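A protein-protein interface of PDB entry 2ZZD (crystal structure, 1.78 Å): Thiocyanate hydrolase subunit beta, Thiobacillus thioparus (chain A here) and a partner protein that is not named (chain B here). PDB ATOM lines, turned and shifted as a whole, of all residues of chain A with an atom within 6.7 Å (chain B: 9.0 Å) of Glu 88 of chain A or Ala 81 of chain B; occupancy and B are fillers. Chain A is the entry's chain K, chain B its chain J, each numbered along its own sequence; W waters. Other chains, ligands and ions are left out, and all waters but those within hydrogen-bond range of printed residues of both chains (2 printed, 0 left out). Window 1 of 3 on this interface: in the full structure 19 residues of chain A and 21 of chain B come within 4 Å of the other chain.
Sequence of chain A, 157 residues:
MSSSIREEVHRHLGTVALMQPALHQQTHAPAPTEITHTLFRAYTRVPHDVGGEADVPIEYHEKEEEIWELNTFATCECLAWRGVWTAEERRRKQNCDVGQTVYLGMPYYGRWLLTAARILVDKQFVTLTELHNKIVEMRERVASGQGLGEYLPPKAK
The backbone NH (N) of Gly 83 of chain B lies close to the side-chain carboxylate (OE2) of Glu 89 of chain A (3.5 Å).
OH of Tyr 53 of chain B is in hydrogen-bond range of OE2 of Glu 88 of chain A, at 2.5 Å.
The backbone carbonyl oxygen (O) of Ala 81 of chain B sits at hydrogen-bond distance from the guanidinium group (NH2) of Arg 92 of chain A (3.0 Å).
NE of Arg 55 of chain B lies within salt-bridge range of OE1 of Glu 88 of chain A (3.4 Å).
The side-chain carboxylate (OE2) of Glu 78 of chain B is in hydrogen-bond range of the backbone NH (N) of Arg 55 of chain B (3.4 Å).
OE1 of Glu 88 of chain A is in salt-bridge range of NH1 of Arg 91 of chain A (3.2 Å).
The side-chain carboxylate (OE1) of Glu 89 of chain A sits at hydrogen-bond distance from the backbone NH (N) of Thr 86 of chain A (2.9 Å).
OH of Tyr 53 of chain B lies within hydrogen-bond range of NH1 of Arg 55 of chain B.
Among the printed residues, merely in contact across the chains: Glu 88 of chain A with Glu 80 of chain B (3.3 Å), Glu 88 of chain A with Ala 77 of chain B (3.4 Å), Arg 91 of chain A with Arg 55 of chain B (3.4 Å), Glu 88 of chain A with Ala 81 of chain B (3.5 Å), Arg 92 of chain A with Phe 82 of chain B (3.5 Å), Glu 89 of chain A with Glu 80 of chain B (3.5 Å), Glu 89 of chain A with Ala 81 of chain B (3.5 Å), Arg 92 of chain A with Tyr 53 of chain B (3.6 Å), Arg 91 of chain A with Tyr 53 of chain B (3.7 Å), Thr 86 of chain A with Glu 85 of chain B (3.7 Å) and Thr 86 of chain A with Glu 80 of chain B (3.9 Å).
Printed residues of chain B within 4 Å of Thr 86 of chain A: Glu 80 (3.9 Å) and Glu 85 (3.7 Å).
Of chain B, only Tyr 53, Arg 55, Ala 77, Glu 80 and Ala 81 come within 4 Å of Glu 88 of chain A.
Of the printed residues of chain B, Arg 92 of chain A touches Tyr 53, Ala 81 and Phe 82.
Asp 79 of chain B touches none of the printed residues of chain A.
Ala 81 of chain B touches just these residues of chain A: Glu 88 (3.5 Å), Glu 89 (3.5 Å) and Arg 92 (3.0 Å).
Of the printed residues of chain A, Glu 85 of chain B touches Thr 86.
Printed residues of chain A that touch a printed residue of chain B: Thr 86, Glu 88, Glu 89, Arg 91 and Arg 92.
Among the printed residues, Asp or Glu carboxylates within 4 Å of a Lys or Arg side-chain nitrogen of the other chain: Glu 88 of chain A with Arg 55 of chain B.
Water W2 lies within hydrogen-bond range of OE2 of Glu 85 of chain B, O of Glu 80 of chain B and OG1 of Thr 86 of chain A.
Water W1 bridges the side-chain carboxylate of Glu 80 of chain B and the backbone NH of Glu 88 of chain A.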
ATOM      1  N   TRP A  85     -20.756  -8.320 -19.484  1.00  0.00           N
ATOM      2  CA  TRP A  85     -20.834  -6.863 -19.379  1.00  0.00           C
ATOM      3  C   TRP A  85     -20.863  -6.212 -20.760  1.00  0.00           C
ATOM      4  O   TRP A  85     -20.641  -6.880 -21.770  1.00  0.00           O
ATOM      5  CB  TRP A  85     -19.650  -6.290 -18.563  1.00  0.00           C
ATOM      6  CG  TRP A  85     -18.235  -6.536 -19.089  1.00  0.00           C
ATOM      7  CD1 TRP A  85     -17.868  -7.154 -20.256  1.00  0.00           C
ATOM      8  CD2 TRP A  85     -17.010  -6.202 -18.414  1.00  0.00           C
ATOM      9  NE1 TRP A  85     -16.492  -7.230 -20.342  1.00  0.00           N
ATOM     10  CE2 TRP A  85     -15.945  -6.655 -19.226  1.00  0.00           C
ATOM     11  CE3 TRP A  85     -16.712  -5.563 -17.201  1.00  0.00           C
ATOM     12  CZ2 TRP A  85     -14.600  -6.497 -18.857  1.00  0.00           C
ATOM     13  CZ3 TRP A  85     -15.369  -5.403 -16.836  1.00  0.00           C
ATOM     14  CH2 TRP A  85     -14.334  -5.871 -17.664  1.00  0.00           C
ATOM     15  N   THR A  86     -21.191  -4.923 -20.802  1.00  0.00           N
ATOM     16  CA  THR A  86     -21.161  -4.173 -22.053  1.00  0.00           C
ATOM     17  C   THR A  86     -19.865  -3.382 -21.913  1.00  0.00           C
ATOM     18  O   THR A  86     -19.325  -3.270 -20.809  1.00  0.00           O
ATOM     19  CB  THR A  86     -22.330  -3.182 -22.200  1.00  0.00           C
ATOM     20  OG1 THR A  86     -22.398  -2.336 -21.043  1.00  0.00           O
ATOM     21  CG2 THR A  86     -23.642  -3.933 -22.390  1.00  0.00           C
ATOM     22  N   ALA A  87     -19.360  -2.838 -23.012  1.00  0.00           N
ATOM     23  CA  ALA A  87     -18.119  -2.086 -22.949  1.00  0.00           C
ATOM     24  C   ALA A  87     -18.244  -0.879 -22.030  1.00  0.00           C
ATOM     25  O   ALA A  87     -17.270  -0.478 -21.396  1.00  0.00           O
ATOM     26  CB  ALA A  87     -17.709  -1.639 -24.339  1.00  0.00           C
ATOM     27  N   GLU A  88     -19.435  -0.291 -21.955  1.00  0.00           N
ATOM     28  CA  GLU A  88     -19.597   0.875 -21.096  1.00  0.00           C
ATOM     29  C   GLU A  88     -19.461   0.504 -19.632  1.00  0.00           C
ATOM     30  O   GLU A  88     -18.893   1.267 -18.850  1.00  0.00           O
ATOM     31  CB  GLU A  88     -20.927   1.586 -21.371  1.00  0.00           C
ATOM     32  CG  GLU A  88     -20.750   2.719 -22.375  1.00  0.00           C
ATOM     33  CD  GLU A  88     -19.735   3.746 -21.894  1.00  0.00           C
ATOM     34  OE1 GLU A  88     -18.810   4.095 -22.661  1.00  0.00           O
ATOM     35  OE2 GLU A  88     -19.867   4.202 -20.740  1.00  0.00           O
ATOM     36  N   GLU A  89     -19.969  -0.664 -19.250  1.00  0.00           N
ATOM     37  CA  GLU A  89     -19.822  -1.089 -17.866  1.00  0.00           C
ATOM     38  C   GLU A  89     -18.322  -1.272 -17.615  1.00  0.00           C
ATOM     39  O   GLU A  89     -17.815  -0.904 -16.557  1.00  0.00           O
ATOM     40  CB  GLU A  89     -20.591  -2.393 -17.614  1.00  0.00           C
ATOM     41  CG  GLU A  89     -22.111  -2.222 -17.687  1.00  0.00           C
ATOM     42  CD  GLU A  89     -22.874  -3.525 -17.510  1.00  0.00           C
ATOM     43  OE1 GLU A  89     -22.580  -4.491 -18.244  1.00  0.00           O
ATOM     44  OE2 GLU A  89     -23.776  -3.581 -16.646  1.00  0.00           O
ATOM     45  N   ARG A  90     -17.605  -1.820 -18.595  1.00  0.00           N
ATOM     46  CA  ARG A  90     -16.161  -2.003 -18.436  1.00  0.00           C
ATOM     47  C   ARG A  90     -15.447  -0.659 -18.247  1.00  0.00           C
ATOM     48  O   ARG A  90     -14.635  -0.506 -17.331  1.00  0.00           O
ATOM     49  CB  ARG A  90     -15.541  -2.727 -19.642  1.00  0.00           C
ATOM     50  CG  ARG A  90     -14.006  -2.800 -19.573  1.00  0.00           C
ATOM     51  CD  ARG A  90     -13.386  -3.576 -20.735  1.00  0.00           C
ATOM     52  NE  ARG A  90     -13.688  -2.974 -22.032  1.00  0.00           N
ATOM     53  CZ  ARG A  90     -13.230  -1.792 -22.441  1.00  0.00           C
ATOM     54  NH1 ARG A  90     -12.435  -1.065 -21.661  1.00  0.00           N
ATOM     55  NH2 ARG A  90     -13.572  -1.330 -23.638  1.00  0.00           N
ATOM     56  N   ARG A  91     -15.741   0.311 -19.111  1.00  0.00           N
ATOM     57  CA  ARG A  91     -15.098   1.623 -19.014  1.00  0.00           C
ATOM     58  C   ARG A  91     -15.314   2.275 -17.659  1.00  0.00           C
ATOM     59  O   ARG A  91     -14.378   2.807 -17.061  1.00  0.00           O
ATOM     60  CB  ARG A  91     -15.608   2.573 -20.097  1.00  0.00           C
ATOM     61  CG  ARG A  91     -15.147   2.193 -21.494  1.00  0.00           C
ATOM     62  CD  ARG A  91     -15.420   3.294 -22.516  1.00  0.00           C
ATOM     63  NE  ARG A  91     -15.114   2.803 -23.852  1.00  0.00           N
ATOM     64  CZ  ARG A  91     -15.963   2.103 -24.598  1.00  0.00           C
ATOM     65  NH1 ARG A  91     -17.187   1.827 -24.148  1.00  0.00           N
ATOM     66  NH2 ARG A  91     -15.573   1.633 -25.777  1.00  0.00           N
ATOM     67  N   ARG A  92     -16.552   2.245 -17.181  1.00  0.00           N
ATOM     68  CA  ARG A  92     -16.866   2.847 -15.898  1.00  0.00           C
ATOM     69  C   ARG A  92     -16.058   2.185 -14.779  1.00  0.00           C
ATOM     70  O   ARG A  92     -15.511   2.866 -13.915  1.00  0.00           O
ATOM     71  CB  ARG A  92     -18.372   2.732 -15.630  1.00  0.00           C
ATOM     72  CG  ARG A  92     -18.838   3.313 -14.300  1.00  0.00           C
ATOM     73  CD  ARG A  92     -18.893   2.241 -13.227  1.00  0.00           C
ATOM     74  NE  ARG A  92     -19.868   1.206 -13.553  1.00  0.00           N
ATOM     75  CZ  ARG A  92     -20.124   0.156 -12.777  1.00  0.00           C
ATOM     76  NH1 ARG A  92     -19.469   0.004 -11.632  1.00  0.00           N
ATOM     77  NH2 ARG A  92     -21.041  -0.736 -13.138  1.00  0.00           N
ATOM     78  N   LYS A  93     -15.963   0.858 -14.807  1.00  0.00           N
ATOM     79  CA  LYS A  93     -15.223   0.131 -13.775  1.00  0.00           C
ATOM     80  C   LYS A  93     -13.703   0.271 -13.905  1.00  0.00           C
ATOM     81  O   LYS A  93     -12.985   0.422 -12.911  1.00  0.00           O
ATOM     82  CB  LYS A  93     -15.577  -1.365 -13.826  1.00  0.00           C
ATOM     83  CG  LYS A  93     -17.031  -1.692 -13.493  1.00  0.00           C
ATOM     84  CD  LYS A  93     -17.314  -3.197 -13.621  1.00  0.00           C
ATOM     85  CE  LYS A  93     -16.688  -3.995 -12.482  1.00  0.00           C
ATOM     86  NZ  LYS A  93     -17.299  -3.640 -11.163  1.00  0.00           N
ATOM     87  N   HIS B  15     -28.193  -8.651 -24.648  1.00  0.00           N
ATOM     88  CA  HIS B  15     -27.525  -7.778 -25.608  1.00  0.00           C
ATOM     89  C   HIS B  15     -27.340  -8.425 -26.981  1.00  0.00           C
ATOM     90  O   HIS B  15     -27.625  -7.806 -28.007  1.00  0.00           O
ATOM     91  CB  HIS B  15     -26.164  -7.326 -25.068  1.00  0.00           C
ATOM     92  CG  HIS B  15     -25.497  -6.282 -25.909  1.00  0.00           C
ATOM     93  ND1 HIS B  15     -25.982  -4.997 -26.026  1.00  0.00           N
ATOM     94  CD2 HIS B  15     -24.390  -6.339 -26.687  1.00  0.00           C
ATOM     95  CE1 HIS B  15     -25.205  -4.307 -26.842  1.00  0.00           C
ATOM     96  NE2 HIS B  15     -24.233  -5.100 -27.259  1.00  0.00           N
ATOM     97  N   ASP B  24     -24.813  -1.963 -32.776  1.00  0.00           N
ATOM     98  CA  ASP B  24     -24.971  -1.031 -31.666  1.00  0.00           C
ATOM     99  C   ASP B  24     -24.239   0.217 -32.166  1.00  0.00           C
ATOM    100  O   ASP B  24     -23.072   0.137 -32.548  1.00  0.00           O
ATOM    101  CB  ASP B  24     -24.270  -1.616 -30.425  1.00  0.00           C
ATOM    102  CG  ASP B  24     -24.383  -0.735 -29.192  1.00  0.00           C
ATOM    103  OD1 ASP B  24     -24.897   0.400 -29.294  1.00  0.00           O
ATOM    104  OD2 ASP B  24     -23.938  -1.195 -28.111  1.00  0.00           O
ATOM    105  N   PHE B  52     -19.711   9.679  -9.745  1.00  0.00           N
ATOM    106  CA  PHE B  52     -19.536   8.296 -10.193  1.00  0.00           C
ATOM    107  C   PHE B  52     -19.248   8.057 -11.674  1.00  0.00           C
ATOM    108  O   PHE B  52     -18.405   7.220 -11.998  1.00  0.00           O
ATOM    109  CB  PHE B  52     -20.727   7.428  -9.760  1.00  0.00           C
ATOM    110  CG  PHE B  52     -21.002   7.461  -8.276  1.00  0.00           C
ATOM    111  CD1 PHE B  52     -19.963   7.623  -7.358  1.00  0.00           C
ATOM    112  CD2 PHE B  52     -22.301   7.314  -7.797  1.00  0.00           C
ATOM    113  CE1 PHE B  52     -20.213   7.636  -5.984  1.00  0.00           C
ATOM    114  CE2 PHE B  52     -22.562   7.324  -6.423  1.00  0.00           C
ATOM    115  CZ  PHE B  52     -21.513   7.487  -5.515  1.00  0.00           C
ATOM    116  N   TYR B  53     -19.936   8.758 -12.574  1.00  0.00           N
ATOM    117  CA  TYR B  53     -19.677   8.563 -14.003  1.00  0.00           C
ATOM    118  C   TYR B  53     -20.289   9.617 -14.920  1.00  0.00           C
ATOM    119  O   TYR B  53     -21.357  10.164 -14.646  1.00  0.00           O
ATOM    120  CB  TYR B  53     -20.182   7.185 -14.457  1.00  0.00           C
ATOM    121  CG  TYR B  53     -19.613   6.704 -15.785  1.00  0.00           C
ATOM    122  CD1 TYR B  53     -18.237   6.549 -15.961  1.00  0.00           C
ATOM    123  CD2 TYR B  53     -20.452   6.375 -16.854  1.00  0.00           C
ATOM    124  CE1 TYR B  53     -17.707   6.077 -17.163  1.00  0.00           C
ATOM    125  CE2 TYR B  53     -19.931   5.899 -18.064  1.00  0.00           C
ATOM    126  CZ  TYR B  53     -18.555   5.755 -18.208  1.00  0.00           C
ATOM    127  OH  TYR B  53     -18.018   5.289 -19.386  1.00  0.00           O
ATOM    128  N   THR B  54     -19.578   9.893 -16.008  1.00  0.00           N
ATOM    129  CA  THR B  54     -20.016  10.819 -17.036  1.00  0.00           C
ATOM    130  C   THR B  54     -19.074  10.694 -18.220  1.00  0.00           C
ATOM    131  O   THR B  54     -17.904  10.346 -18.064  1.00  0.00           O
ATOM    132  CB  THR B  54     -19.997  12.298 -16.585  1.00  0.00           C
ATOM    133  OG1 THR B  54     -20.584  13.108 -17.616  1.00  0.00           O
ATOM    134  CG2 THR B  54     -18.566  12.786 -16.349  1.00  0.00           C
ATOM    135  N   ARG B  55     -19.600  10.944 -19.411  1.00  0.00           N
ATOM    136  CA  ARG B  55     -18.782  10.913 -20.602  1.00  0.00           C
ATOM    137  C   ARG B  55     -18.896  12.269 -21.298  1.00  0.00           C
ATOM    138  O   ARG B  55     -18.592  12.410 -22.479  1.00  0.00           O
ATOM    139  CB  ARG B  55     -19.187   9.757 -21.522  1.00  0.00           C
ATOM    140  CG  ARG B  55     -18.844   8.385 -20.926  1.00  0.00           C
ATOM    141  CD  ARG B  55     -18.844   7.273 -21.981  1.00  0.00           C
ATOM    142  NE  ARG B  55     -17.680   7.322 -22.870  1.00  0.00           N
ATOM    143  CZ  ARG B  55     -16.458   6.905 -22.534  1.00  0.00           C
ATOM    144  NH1 ARG B  55     -16.224   6.400 -21.323  1.00  0.00           N
ATOM    145  NH2 ARG B  55     -15.460   6.991 -23.408  1.00  0.00           N
ATOM    146  N   SER B  74     -29.231   6.231 -28.452  1.00  0.00           N
ATOM    147  CA  SER B  74     -28.634   5.232 -27.577  1.00  0.00           C
ATOM    148  C   SER B  74     -28.886   5.563 -26.116  1.00  0.00           C
ATOM    149  O   SER B  74     -29.241   6.693 -25.778  1.00  0.00           O
ATOM    150  CB  SER B  74     -27.121   5.181 -27.808  1.00  0.00           C
ATOM    151  OG  SER B  74     -26.458   4.458 -26.780  1.00  0.00           O
ATOM    152  N   PRO B  75     -28.777   4.559 -25.231  1.00  0.00           N
ATOM    153  CA  PRO B  75     -28.994   4.906 -23.827  1.00  0.00           C
ATOM    154  C   PRO B  75     -27.792   5.804 -23.515  1.00  0.00           C
ATOM    155  O   PRO B  75     -26.754   5.690 -24.165  1.00  0.00           O
ATOM    156  CB  PRO B  75     -28.873   3.560 -23.115  1.00  0.00           C
ATOM    157  CG  PRO B  75     -29.372   2.584 -24.144  1.00  0.00           C
ATOM    158  CD  PRO B  75     -28.729   3.096 -25.413  1.00  0.00           C
ATOM    159  N   ALA B  76     -27.928   6.700 -22.546  1.00  0.00           N
ATOM    160  CA  ALA B  76     -26.807   7.552 -22.192  1.00  0.00           C
ATOM    161  C   ALA B  76     -25.786   6.644 -21.501  1.00  0.00           C
ATOM    162  O   ALA B  76     -26.164   5.670 -20.851  1.00  0.00           O
ATOM    163  CB  ALA B  76     -27.256   8.659 -21.252  1.00  0.00           C
ATOM    164  N   ALA B  77     -24.499   6.948 -21.644  1.00  0.00           N
ATOM    165  CA  ALA B  77     -23.468   6.125 -21.017  1.00  0.00           C
ATOM    166  C   ALA B  77     -23.665   6.088 -19.508  1.00  0.00           C
ATOM    167  O   ALA B  77     -23.368   5.086 -18.853  1.00  0.00           O
ATOM    168  CB  ALA B  77     -22.080   6.666 -21.356  1.00  0.00           C
ATOM    169  N   GLU B  78     -24.163   7.191 -18.960  1.00  0.00           N
ATOM    170  CA  GLU B  78     -24.406   7.296 -17.529  1.00  0.00           C
ATOM    171  C   GLU B  78     -25.367   6.200 -17.056  1.00  0.00           C
ATOM    172  O   GLU B  78     -25.359   5.814 -15.886  1.00  0.00           O
ATOM    173  CB  GLU B  78     -24.968   8.680 -17.184  1.00  0.00           C
ATOM    174  CG  GLU B  78     -23.954   9.830 -17.287  1.00  0.00           C
ATOM    175  CD  GLU B  78     -23.679  10.283 -18.717  1.00  0.00           C
ATOM    176  OE1 GLU B  78     -24.240   9.688 -19.658  1.00  0.00           O
ATOM    177  OE2 GLU B  78     -22.898  11.243 -18.898  1.00  0.00           O
ATOM    178  N   ASP B  79     -26.197   5.701 -17.967  1.00  0.00           N
ATOM    179  CA  ASP B  79     -27.135   4.636 -17.630  1.00  0.00           C
ATOM    180  C   ASP B  79     -26.612   3.276 -18.090  1.00  0.00           C
ATOM    181  O   ASP B  79     -26.647   2.295 -17.345  1.00  0.00           O
ATOM    182  CB  ASP B  79     -28.512   4.904 -18.257  1.00  0.00           C
ATOM    183  CG  ASP B  79     -29.244   6.046 -17.578  1.00  0.00           C
ATOM    184  OD1 ASP B  79     -29.138   6.156 -16.336  1.00  0.00           O
ATOM    185  OD2 ASP B  79     -29.931   6.823 -18.275  1.00  0.00           O
ATOM    186  N   GLU B  80     -26.111   3.230 -19.317  1.00  0.00           N
ATOM    187  CA  GLU B  80     -25.592   1.996 -19.880  1.00  0.00           C
ATOM    188  C   GLU B  80     -24.471   1.406 -19.023  1.00  0.00           C
ATOM    189  O   GLU B  80     -24.389   0.193 -18.853  1.00  0.00           O
ATOM    190  CB  GLU B  80     -25.088   2.260 -21.303  1.00  0.00           C
ATOM    191  CG  GLU B  80     -24.974   1.024 -22.181  1.00  0.00           C
ATOM    192  CD  GLU B  80     -24.664   1.379 -23.622  1.00  0.00           C
ATOM    193  OE1 GLU B  80     -23.644   2.063 -23.851  1.00  0.00           O
ATOM    194  OE2 GLU B  80     -25.438   0.981 -24.523  1.00  0.00           O
ATOM    195  N   ALA B  81     -23.623   2.269 -18.469  1.00  0.00           N
ATOM    196  CA  ALA B  81     -22.499   1.823 -17.646  1.00  0.00           C
ATOM    197  C   ALA B  81     -22.911   1.195 -16.316  1.00  0.00           C
ATOM    198  O   ALA B  81     -22.072   0.639 -15.606  1.00  0.00           O
ATOM    199  CB  ALA B  81     -21.543   2.988 -17.391  1.00  0.00           C
ATOM    200  N   PHE B  82     -24.190   1.296 -15.967  1.00  0.00           N
ATOM    201  CA  PHE B  82     -24.669   0.709 -14.723  1.00  0.00           C
ATOM    202  C   PHE B  82     -25.745  -0.337 -14.992  1.00  0.00           C
ATOM    203  O   PHE B  82     -26.476  -0.745 -14.088  1.00  0.00           O
ATOM    204  CB  PHE B  82     -25.157   1.813 -13.775  1.00  0.00           C
ATOM    205  CG  PHE B  82     -24.027   2.553 -13.108  1.00  0.00           C
ATOM    206  CD1 PHE B  82     -23.367   1.991 -12.016  1.00  0.00           C
ATOM    207  CD2 PHE B  82     -23.562   3.762 -13.626  1.00  0.00           C
ATOM    208  CE1 PHE B  82     -22.255   2.615 -11.447  1.00  0.00           C
ATOM    209  CE2 PHE B  82     -22.451   4.396 -13.068  1.00  0.00           C
ATOM    210  CZ  PHE B  82     -21.795   3.822 -11.976  1.00  0.00           C
ATOM    211  N   GLY B  83     -25.809  -0.775 -16.248  1.00  0.00           N
ATOM    212  CA  GLY B  83     -26.757  -1.799 -16.654  1.00  0.00           C
ATOM    213  C   GLY B  83     -28.183  -1.343 -16.889  1.00  0.00           C
ATOM    214  O   GLY B  83     -29.090  -2.170 -16.957  1.00  0.00           O
ATOM    215  N   ASN B  84     -28.377  -0.038 -17.035  1.00  0.00           N
ATOM    216  CA  ASN B  84     -29.703   0.537 -17.236  1.00  0.00           C
ATOM    217  C   ASN B  84     -29.866   1.001 -18.680  1.00  0.00           C
ATOM    218  O   ASN B  84     -29.361   2.053 -19.057  1.00  0.00           O
ATOM    219  CB  ASN B  84     -29.885   1.712 -16.274  1.00  0.00           C
ATOM    220  CG  ASN B  84     -29.619   1.323 -14.829  1.00  0.00           C
ATOM    221  OD1 ASN B  84     -28.877   2.002 -14.111  1.00  0.00           O
ATOM    222  ND2 ASN B  84     -30.230   0.229 -14.391  1.00  0.00           N
ATOM    223  N   GLU B  85     -30.584   0.220 -19.484  1.00  0.00           N
ATOM    224  CA  GLU B  85     -30.771   0.564 -20.894  1.00  0.00           C
ATOM    225  C   GLU B  85     -32.223   0.846 -21.292  1.00  0.00           C
ATOM    226  O   GLU B  85     -32.536   0.926 -22.486  1.00  0.00           O
ATOM    227  CB  GLU B  85     -30.211  -0.560 -21.772  1.00  0.00           C
ATOM    228  CG  GLU B  85     -28.744  -0.880 -21.490  1.00  0.00           C
ATOM    229  CD  GLU B  85     -28.189  -1.959 -22.403  1.00  0.00           C
ATOM    230  OE1 GLU B  85     -28.970  -2.538 -23.194  1.00  0.00           O
ATOM    231  OE2 GLU B  85     -26.972  -2.230 -22.320  1.00  0.00           O
ATOM    232  N   PHE B  91     -28.218  11.499 -29.587  1.00  0.00           N
ATOM    233  CA  PHE B  91     -26.841  11.945 -29.396  1.00  0.00           C
ATOM    234  C   PHE B  91     -26.540  12.943 -30.508  1.00  0.00           C
ATOM    235  O   PHE B  91     -26.936  12.746 -31.659  1.00  0.00           O
ATOM    236  CB  PHE B  91     -25.854  10.779 -29.460  1.00  0.00           C
ATOM    237  CG  PHE B  91     -25.703  10.038 -28.155  1.00  0.00           C
ATOM    238  CD1 PHE B  91     -26.794   9.419 -27.560  1.00  0.00           C
ATOM    239  CD2 PHE B  91     -24.460   9.947 -27.533  1.00  0.00           C
ATOM    240  CE1 PHE B  91     -26.652   8.714 -26.362  1.00  0.00           C
ATOM    241  CE2 PHE B  91     -24.301   9.245 -26.337  1.00  0.00           C
ATOM    242  CZ  PHE B  91     -25.401   8.626 -25.748  1.00  0.00           C
HETATM  243  O   HOH W   1     -21.690  -0.020 -24.213  1.00  0.00           O
HETATM  244  O   HOH W   2     -25.236  -2.060 -20.225  1.00  0.00           O
